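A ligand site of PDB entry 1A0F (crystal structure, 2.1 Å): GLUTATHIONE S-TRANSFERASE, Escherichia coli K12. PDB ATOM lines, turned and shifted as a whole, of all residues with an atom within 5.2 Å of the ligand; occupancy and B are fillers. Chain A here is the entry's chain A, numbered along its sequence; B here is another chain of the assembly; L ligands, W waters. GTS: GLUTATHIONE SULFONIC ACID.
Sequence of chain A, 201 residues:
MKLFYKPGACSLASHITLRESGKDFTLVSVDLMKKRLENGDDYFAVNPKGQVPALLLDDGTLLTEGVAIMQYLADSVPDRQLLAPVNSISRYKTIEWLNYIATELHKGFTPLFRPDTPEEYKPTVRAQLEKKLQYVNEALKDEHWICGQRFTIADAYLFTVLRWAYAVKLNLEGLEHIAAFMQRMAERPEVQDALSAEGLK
O2S of the ligand sits at hydrogen-bond distance from N of Cys 10 (2.9 Å). ND2 of Asn 99 of chain B sits at hydrogen-bond distance from O11 of the ligand. The side-chain hydroxyl of Thr 103 of chain B is in hydrogen-bond range of a nitrogen (N1) of the ligand (2.8 Å). The backbone carbonyl oxygen (O) of Val 52 is in hydrogen-bond range of a nitrogen (N2) of the ligand (2.8 Å). O31 of the ligand is in salt-bridge range of NZ of Lys 35. N1 of the ligand is in salt-bridge range of OE1 of Glu 65 (2.6 Å). An oxygen (O2) of the ligand sits at hydrogen-bond distance from the backbone NH of Val 52, 2.8 Å away. An oxygen (O1S) of the ligand sits at hydrogen-bond distance from the side-chain sulfur (SG) of Cys 10 (2.9 Å). NE2 of His 106 is in hydrogen-bond range of O1S of the ligand. N of Gly 66 is in hydrogen-bond range of O12 of the ligand (3.0 Å). A nitrogen (N1) of the ligand lies within salt-bridge range of the side-chain carboxylate (OE2) of Glu 104 of chain B (2.8 Å).
The indole nitrogen (NE1) of Trp 164 is in hydrogen-bond range of the backbone carbonyl oxygen (O) of Gly 8 (3.1 Å). The side-chain amino group (NZ) of Lys 107 is in salt-bridge range of the side-chain carboxylate (OE2) of Glu 104 of chain B. The side-chain hydroxyl (OG1) of Thr 103 of chain B lies within hydrogen-bond range of the backbone carbonyl oxygen (O) of Asn 99 of chain B (2.6 Å). The side-chain amino group (NZ) of Lys 35 sits at hydrogen-bond distance from the backbone carbonyl oxygen (O) of Leu 32, at 3.0 Å. The side-chain carboxylate (OE2) of Glu 104 of chain B lies within hydrogen-bond range of the side-chain amide nitrogen (NE2) of Gln 51 (3.5 Å). OH of Tyr 157 lies within hydrogen-bond range of ND1 of His 106 (2.7 Å). O of Val 52 is in hydrogen-bond range of SG of Cys 10 (3.4 Å). The side-chain carboxylate of Glu 65 sits at hydrogen-bond distance from the side-chain amide nitrogen of Asn 99 of chain B, at 3.0 Å.
Ala 9 touches the ligand (CB to O2S, 3.1 Å). Leu 32 touches the ligand. CA of Gln 51 touches O2 of the ligand (3.0 Å). NZ of Lys 107 touches OE1 of the ligand, 3.6 Å away. Trp 164 touches the ligand (CZ2 to O2S, 3.8 Å). Hydrophobic or aromatic side chains that line the ligand: Ala 9, Leu 32, Val 52, His 106 and Trp 164. Within 4 Å of the ligand: Ala 9, Cys 10, Leu 32, Lys 35, Gln 51, Val 52, Glu 65, Gly 66, His 106, Lys 107, Trp 164, Asn 99 of chain B, Thr 103 of chain B and Glu 104 of chain B. The nearest printed residue that does not touch the ligand is Pro 53 (4.02 Å).
Water W5 lies within hydrogen-bond range of O11 of the ligand, OH of Tyr 157, N of Val 67 and N of Gly 66. Water W4 lies within hydrogen-bond range of O of Pro 53 (2.7 Å), O12 of the ligand (2.9 Å) and N of Glu 65 (2.9 Å). Water W1 lies within hydrogen-bond range of the side-chain amide oxygen of Gln 51 (2.5 Å), the side-chain carboxylate of Glu 65 (2.6 Å) and a nitrogen (N1) of the ligand (3.4 Å).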
ATOM      1  N   GLY A   8     -24.645   6.720 -16.137  1.00  0.00           N
ATOM      2  CA  GLY A   8     -25.117   5.819 -17.176  1.00  0.00           C
ATOM      3  C   GLY A   8     -24.264   4.606 -17.530  1.00  0.00           C
ATOM      4  O   GLY A   8     -24.751   3.626 -18.097  1.00  0.00           O
ATOM      5  N   ALA A   9     -22.984   4.682 -17.197  1.00  0.00           N
ATOM      6  CA  ALA A   9     -22.075   3.588 -17.460  1.00  0.00           C
ATOM      7  C   ALA A   9     -22.566   2.354 -16.672  1.00  0.00           C
ATOM      8  O   ALA A   9     -23.580   2.418 -16.007  1.00  0.00           O
ATOM      9  CB  ALA A   9     -20.654   4.027 -17.009  1.00  0.00           C
ATOM     10  N   CYS A  10     -21.834   1.257 -16.707  1.00  0.00           N
ATOM     11  CA  CYS A  10     -22.207   0.017 -15.998  1.00  0.00           C
ATOM     12  C   CYS A  10     -22.208   0.106 -14.452  1.00  0.00           C
ATOM     13  O   CYS A  10     -22.775  -0.754 -13.768  1.00  0.00           O
ATOM     14  CB  CYS A  10     -21.300  -1.118 -16.459  1.00  0.00           C
ATOM     15  SG  CYS A  10     -19.522  -1.012 -15.923  1.00  0.00           S
ATOM     16  N   LEU A  32     -13.701   9.342 -17.986  1.00  0.00           N
ATOM     17  CA  LEU A  32     -13.177   8.149 -18.622  1.00  0.00           C
ATOM     18  C   LEU A  32     -12.280   8.337 -19.846  1.00  0.00           C
ATOM     19  O   LEU A  32     -11.565   7.421 -20.212  1.00  0.00           O
ATOM     20  CB  LEU A  32     -14.291   7.127 -18.893  1.00  0.00           C
ATOM     21  CG  LEU A  32     -14.939   6.425 -17.688  1.00  0.00           C
ATOM     22  CD1 LEU A  32     -15.886   5.351 -18.193  1.00  0.00           C
ATOM     23  CD2 LEU A  32     -13.913   5.790 -16.764  1.00  0.00           C
ATOM     24  N   LYS A  35      -9.147   9.723 -17.758  1.00  0.00           N
ATOM     25  CA  LYS A  35      -8.800   8.971 -16.561  1.00  0.00           C
ATOM     26  C   LYS A  35      -8.406   9.914 -15.446  1.00  0.00           C
ATOM     27  O   LYS A  35      -7.377   9.724 -14.778  1.00  0.00           O
ATOM     28  CB  LYS A  35      -7.639   8.023 -16.835  1.00  0.00           C
ATOM     29  CG  LYS A  35      -8.081   6.618 -17.049  1.00  0.00           C
ATOM     30  CD  LYS A  35      -8.867   6.473 -18.335  1.00  0.00           C
ATOM     31  CE  LYS A  35      -9.226   5.012 -18.548  1.00  0.00           C
ATOM     32  NZ  LYS A  35     -10.101   4.834 -19.698  1.00  0.00           N
ATOM     33  N   GLY A  50      -8.294   1.437 -14.910  1.00  0.00           N
ATOM     34  CA  GLY A  50      -8.900   2.616 -15.516  1.00  0.00           C
ATOM     35  C   GLY A  50     -10.364   2.584 -15.840  1.00  0.00           C
ATOM     36  O   GLY A  50     -10.856   3.416 -16.565  1.00  0.00           O
ATOM     37  N   GLN A  51     -11.086   1.636 -15.257  1.00  0.00           N
ATOM     38  CA  GLN A  51     -12.501   1.468 -15.518  1.00  0.00           C
ATOM     39  C   GLN A  51     -13.436   1.721 -14.327  1.00  0.00           C
ATOM     40  O   GLN A  51     -13.042   1.574 -13.159  1.00  0.00           O
ATOM     41  CB  GLN A  51     -12.758   0.012 -15.915  1.00  0.00           C
ATOM     42  CG  GLN A  51     -11.945  -0.529 -17.030  1.00  0.00           C
ATOM     43  CD  GLN A  51     -12.119  -2.010 -17.120  1.00  0.00           C
ATOM     44  OE1 GLN A  51     -12.165  -2.682 -16.102  1.00  0.00           O
ATOM     45  NE2 GLN A  51     -12.254  -2.521 -18.326  1.00  0.00           N
ATOM     46  N   VAL A  52     -14.688   2.056 -14.643  1.00  0.00           N
ATOM     47  CA  VAL A  52     -15.704   2.191 -13.609  1.00  0.00           C
ATOM     48  C   VAL A  52     -16.528   0.910 -13.769  1.00  0.00           C
ATOM     49  O   VAL A  52     -16.598   0.332 -14.828  1.00  0.00           O
ATOM     50  CB  VAL A  52     -16.565   3.461 -13.759  1.00  0.00           C
ATOM     51  CG1 VAL A  52     -15.662   4.663 -13.587  1.00  0.00           C
ATOM     52  CG2 VAL A  52     -17.295   3.481 -15.062  1.00  0.00           C
ATOM     53  N   PRO A  53     -17.054   0.390 -12.673  1.00  0.00           N
ATOM     54  CA  PRO A  53     -16.939   0.892 -11.312  1.00  0.00           C
ATOM     55  C   PRO A  53     -15.760   0.358 -10.518  1.00  0.00           C
ATOM     56  O   PRO A  53     -15.165  -0.677 -10.861  1.00  0.00           O
ATOM     57  CB  PRO A  53     -18.212   0.383 -10.678  1.00  0.00           C
ATOM     58  CG  PRO A  53     -18.305  -1.003 -11.298  1.00  0.00           C
ATOM     59  CD  PRO A  53     -18.009  -0.724 -12.757  1.00  0.00           C
ATOM     60  N   GLU A  65     -14.570  -4.582 -10.581  1.00  0.00           N
ATOM     61  CA  GLU A  65     -15.459  -5.546 -11.223  1.00  0.00           C
ATOM     62  C   GLU A  65     -16.862  -5.478 -10.616  1.00  0.00           C
ATOM     63  O   GLU A  65     -17.061  -5.876  -9.476  1.00  0.00           O
ATOM     64  CB  GLU A  65     -14.933  -6.972 -11.131  1.00  0.00           C
ATOM     65  CG  GLU A  65     -13.494  -7.149 -11.637  1.00  0.00           C
ATOM     66  CD  GLU A  65     -13.350  -6.809 -13.095  1.00  0.00           C
ATOM     67  OE1 GLU A  65     -14.301  -7.011 -13.875  1.00  0.00           O
ATOM     68  OE2 GLU A  65     -12.285  -6.343 -13.482  1.00  0.00           O
ATOM     69  N   GLY A  66     -17.820  -4.995 -11.403  1.00  0.00           N
ATOM     70  CA  GLY A  66     -19.188  -4.864 -10.922  1.00  0.00           C
ATOM     71  C   GLY A  66     -19.771  -6.069 -10.217  1.00  0.00           C
ATOM     72  O   GLY A  66     -20.294  -5.951  -9.101  1.00  0.00           O
ATOM     73  N   VAL A  67     -19.696  -7.230 -10.849  1.00  0.00           N
ATOM     74  CA  VAL A  67     -20.190  -8.475 -10.280  1.00  0.00           C
ATOM     75  C   VAL A  67     -19.577  -8.755  -8.899  1.00  0.00           C
ATOM     76  O   VAL A  67     -20.291  -9.219  -8.013  1.00  0.00           O
ATOM     77  CB  VAL A  67     -19.950  -9.649 -11.267  1.00  0.00           C
ATOM     78  CG1 VAL A  67     -20.209 -10.982 -10.630  1.00  0.00           C
ATOM     79  CG2 VAL A  67     -20.853  -9.489 -12.447  1.00  0.00           C
ATOM     80  N   HIS A 106     -23.449  -7.069 -21.447  1.00  0.00           N
ATOM     81  CA  HIS A 106     -22.539  -5.934 -21.176  1.00  0.00           C
ATOM     82  C   HIS A 106     -21.335  -5.924 -22.160  1.00  0.00           C
ATOM     83  O   HIS A 106     -21.138  -4.953 -22.915  1.00  0.00           O
ATOM     84  CB  HIS A 106     -22.064  -6.033 -19.699  1.00  0.00           C
ATOM     85  CG  HIS A 106     -21.107  -4.947 -19.267  1.00  0.00           C
ATOM     86  ND1 HIS A 106     -20.629  -4.874 -17.972  1.00  0.00           N
ATOM     87  CD2 HIS A 106     -20.555  -3.907 -19.922  1.00  0.00           C
ATOM     88  CE1 HIS A 106     -19.837  -3.829 -17.850  1.00  0.00           C
ATOM     89  NE2 HIS A 106     -19.776  -3.225 -19.026  1.00  0.00           N
ATOM     90  N   LYS A 107     -20.558  -7.009 -22.165  1.00  0.00           N
ATOM     91  CA  LYS A 107     -19.410  -7.093 -23.044  1.00  0.00           C
ATOM     92  C   LYS A 107     -19.828  -7.206 -24.498  1.00  0.00           C
ATOM     93  O   LYS A 107     -19.065  -6.899 -25.408  1.00  0.00           O
ATOM     94  CB  LYS A 107     -18.471  -8.232 -22.631  1.00  0.00           C
ATOM     95  CG  LYS A 107     -17.681  -7.868 -21.396  1.00  0.00           C
ATOM     96  CD  LYS A 107     -16.709  -6.752 -21.718  1.00  0.00           C
ATOM     97  CE  LYS A 107     -16.530  -5.796 -20.587  1.00  0.00           C
ATOM     98  NZ  LYS A 107     -15.314  -5.003 -20.884  1.00  0.00           N
ATOM     99  N   PHE A 113     -19.800   0.799 -28.516  1.00  0.00           N
ATOM    100  CA  PHE A 113     -19.353   2.005 -27.822  1.00  0.00           C
ATOM    101  C   PHE A 113     -17.860   2.341 -28.027  1.00  0.00           C
ATOM    102  O   PHE A 113     -17.303   3.184 -27.322  1.00  0.00           O
ATOM    103  CB  PHE A 113     -19.625   1.835 -26.330  1.00  0.00           C
ATOM    104  CG  PHE A 113     -21.080   1.546 -25.989  1.00  0.00           C
ATOM    105  CD1 PHE A 113     -22.101   1.734 -26.915  1.00  0.00           C
ATOM    106  CD2 PHE A 113     -21.440   1.133 -24.701  1.00  0.00           C
ATOM    107  CE1 PHE A 113     -23.439   1.519 -26.577  1.00  0.00           C
ATOM    108  CE2 PHE A 113     -22.780   0.910 -24.342  1.00  0.00           C
ATOM    109  CZ  PHE A 113     -23.774   1.110 -25.289  1.00  0.00           C
ATOM    110  N   TYR A 157     -28.387  -5.194 -12.425  1.00  0.00           N
ATOM    111  CA  TYR A 157     -27.424  -5.277 -13.547  1.00  0.00           C
ATOM    112  C   TYR A 157     -28.132  -5.459 -14.887  1.00  0.00           C
ATOM    113  O   TYR A 157     -27.706  -4.889 -15.873  1.00  0.00           O
ATOM    114  CB  TYR A 157     -26.470  -6.427 -13.302  1.00  0.00           C
ATOM    115  CG  TYR A 157     -25.210  -6.442 -14.100  1.00  0.00           C
ATOM    116  CD1 TYR A 157     -24.787  -5.337 -14.843  1.00  0.00           C
ATOM    117  CD2 TYR A 157     -24.373  -7.571 -14.046  1.00  0.00           C
ATOM    118  CE1 TYR A 157     -23.556  -5.331 -15.490  1.00  0.00           C
ATOM    119  CE2 TYR A 157     -23.137  -7.573 -14.691  1.00  0.00           C
ATOM    120  CZ  TYR A 157     -22.730  -6.468 -15.397  1.00  0.00           C
ATOM    121  OH  TYR A 157     -21.498  -6.487 -16.001  1.00  0.00           O
ATOM    122  N   TRP A 164     -29.071   0.584 -22.235  1.00  0.00           N
ATOM    123  CA  TRP A 164     -28.304   0.817 -23.482  1.00  0.00           C
ATOM    124  C   TRP A 164     -28.994   0.258 -24.730  1.00  0.00           C
ATOM    125  O   TRP A 164     -28.754   0.731 -25.819  1.00  0.00           O
ATOM    126  CB  TRP A 164     -26.920   0.194 -23.427  1.00  0.00           C
ATOM    127  CG  TRP A 164     -26.105   0.604 -22.268  1.00  0.00           C
ATOM    128  CD1 TRP A 164     -26.327   1.657 -21.416  1.00  0.00           C
ATOM    129  CD2 TRP A 164     -24.963  -0.089 -21.753  1.00  0.00           C
ATOM    130  NE1 TRP A 164     -25.413   1.638 -20.415  1.00  0.00           N
ATOM    131  CE2 TRP A 164     -24.557   0.583 -20.592  1.00  0.00           C
ATOM    132  CE3 TRP A 164     -24.256  -1.230 -22.169  1.00  0.00           C
ATOM    133  CZ2 TRP A 164     -23.470   0.152 -19.825  1.00  0.00           C
ATOM    134  CZ3 TRP A 164     -23.176  -1.644 -21.415  1.00  0.00           C
ATOM    135  CH2 TRP A 164     -22.792  -0.962 -20.253  1.00  0.00           C
ATOM    136  N   ASN B  99     -14.287 -12.579 -12.653  1.00  0.00           N
ATOM    137  CA  ASN B  99     -15.008 -11.687 -13.563  1.00  0.00           C
ATOM    138  C   ASN B  99     -14.042 -10.988 -14.491  1.00  0.00           C
ATOM    139  O   ASN B  99     -14.416 -10.663 -15.584  1.00  0.00           O
ATOM    140  CB  ASN B  99     -15.873 -10.647 -12.824  1.00  0.00           C
ATOM    141  CG  ASN B  99     -16.920 -10.010 -13.735  1.00  0.00           C
ATOM    142  OD1 ASN B  99     -17.822 -10.697 -14.217  1.00  0.00           O
ATOM    143  ND2 ASN B  99     -16.782  -8.708 -14.011  1.00  0.00           N
ATOM    144  N   TYR B 100     -12.843 -10.672 -14.017  1.00  0.00           N
ATOM    145  CA  TYR B 100     -11.880 -10.068 -14.925  1.00  0.00           C
ATOM    146  C   TYR B 100     -11.561 -11.080 -16.039  1.00  0.00           C
ATOM    147  O   TYR B 100     -11.539 -10.721 -17.222  1.00  0.00           O
ATOM    148  CB  TYR B 100     -10.619  -9.691 -14.184  1.00  0.00           C
ATOM    149  CG  TYR B 100      -9.540  -9.226 -15.119  1.00  0.00           C
ATOM    150  CD1 TYR B 100      -9.469  -7.909 -15.543  1.00  0.00           C
ATOM    151  CD2 TYR B 100      -8.587 -10.121 -15.612  1.00  0.00           C
ATOM    152  CE1 TYR B 100      -8.486  -7.482 -16.434  1.00  0.00           C
ATOM    153  CE2 TYR B 100      -7.599  -9.703 -16.501  1.00  0.00           C
ATOM    154  CZ  TYR B 100      -7.564  -8.394 -16.918  1.00  0.00           C
ATOM    155  OH  TYR B 100      -6.635  -8.004 -17.865  1.00  0.00           O
ATOM    156  N   THR B 103     -14.941 -11.601 -18.441  1.00  0.00           N
ATOM    157  CA  THR B 103     -15.271 -10.450 -19.268  1.00  0.00           C
ATOM    158  C   THR B 103     -14.163  -9.840 -20.092  1.00  0.00           C
ATOM    159  O   THR B 103     -14.416  -9.447 -21.219  1.00  0.00           O
ATOM    160  CB  THR B 103     -15.913  -9.304 -18.432  1.00  0.00           C
ATOM    161  OG1 THR B 103     -14.994  -8.892 -17.424  1.00  0.00           O
ATOM    162  CG2 THR B 103     -17.210  -9.749 -17.731  1.00  0.00           C
ATOM    163  N   GLU B 104     -12.935  -9.808 -19.564  1.00  0.00           N
ATOM    164  CA  GLU B 104     -11.800  -9.193 -20.246  1.00  0.00           C
ATOM    165  C   GLU B 104     -10.918 -10.124 -21.031  1.00  0.00           C
ATOM    166  O   GLU B 104     -10.401  -9.746 -22.046  1.00  0.00           O
ATOM    167  CB  GLU B 104     -10.919  -8.435 -19.262  1.00  0.00           C
ATOM    168  CG  GLU B 104     -11.667  -7.418 -18.386  1.00  0.00           C
ATOM    169  CD  GLU B 104     -12.362  -6.310 -19.184  1.00  0.00           C
ATOM    170  OE1 GLU B 104     -11.898  -5.938 -20.276  1.00  0.00           O
ATOM    171  OE2 GLU B 104     -13.390  -5.787 -18.727  1.00  0.00           O
HETATM  172  N1  GTS L   1     -14.813  -6.263 -16.351  1.00  0.00           N
HETATM  173  CA1 GTS L   1     -15.269  -4.924 -15.879  1.00  0.00           C
HETATM  174  C1  GTS L   1     -16.454  -5.093 -14.997  1.00  0.00           C
HETATM  175  O11 GTS L   1     -17.245  -6.066 -15.216  1.00  0.00           O
HETATM  176  O12 GTS L   1     -16.613  -4.259 -14.066  1.00  0.00           O
HETATM  177  CB1 GTS L   1     -15.552  -3.990 -17.047  1.00  0.00           C
HETATM  178  CG1 GTS L   1     -15.845  -2.546 -16.613  1.00  0.00           C
HETATM  179  CD1 GTS L   1     -16.098  -1.617 -17.779  1.00  0.00           C
HETATM  180  OE1 GTS L   1     -16.086  -2.085 -18.943  1.00  0.00           O
HETATM  181  N2  GTS L   1     -16.316  -0.329 -17.522  1.00  0.00           N
HETATM  182  CA2 GTS L   1     -16.296   0.665 -18.547  1.00  0.00           C
HETATM  183  C2  GTS L   1     -15.112   1.567 -18.531  1.00  0.00           C
HETATM  184  O2  GTS L   1     -14.738   2.000 -17.463  1.00  0.00           O
HETATM  185  CB2 GTS L   1     -17.570   1.514 -18.422  1.00  0.00           C
HETATM  186  SG2 GTS L   1     -18.964   0.855 -19.223  1.00  0.00           S
HETATM  187  O1S GTS L   1     -19.209  -0.540 -18.722  1.00  0.00           O
HETATM  188  O2S GTS L   1     -20.153   1.695 -18.973  1.00  0.00           O
HETATM  189  O3S GTS L   1     -18.707   0.803 -20.691  1.00  0.00           O
HETATM  190  N3  GTS L   1     -14.515   1.855 -19.664  1.00  0.00           N
HETATM  191  CA3 GTS L   1     -13.358   2.716 -19.790  1.00  0.00           C
HETATM  192  C3  GTS L   1     -12.186   1.919 -20.438  1.00  0.00           C
HETATM  193  O31 GTS L   1     -11.237   2.569 -20.906  1.00  0.00           O
HETATM  194  O32 GTS L   1     -12.270   0.670 -20.465  1.00  0.00           O
HETATM  195  O   HOH W   1     -11.628  -5.121 -15.690  1.00  0.00           O
HETATM  196  O   HOH W   2     -12.707  -0.948 -23.445  1.00  0.00           O
HETATM  197  O   HOH W   3     -15.141   0.151 -22.519  1.00  0.00           O
HETATM  198  O   HOH W   4     -14.688  -2.583 -12.711  1.00  0.00           O
HETATM  199  O   HOH W   5     -19.465  -6.451 -13.898  1.00  0.00           O
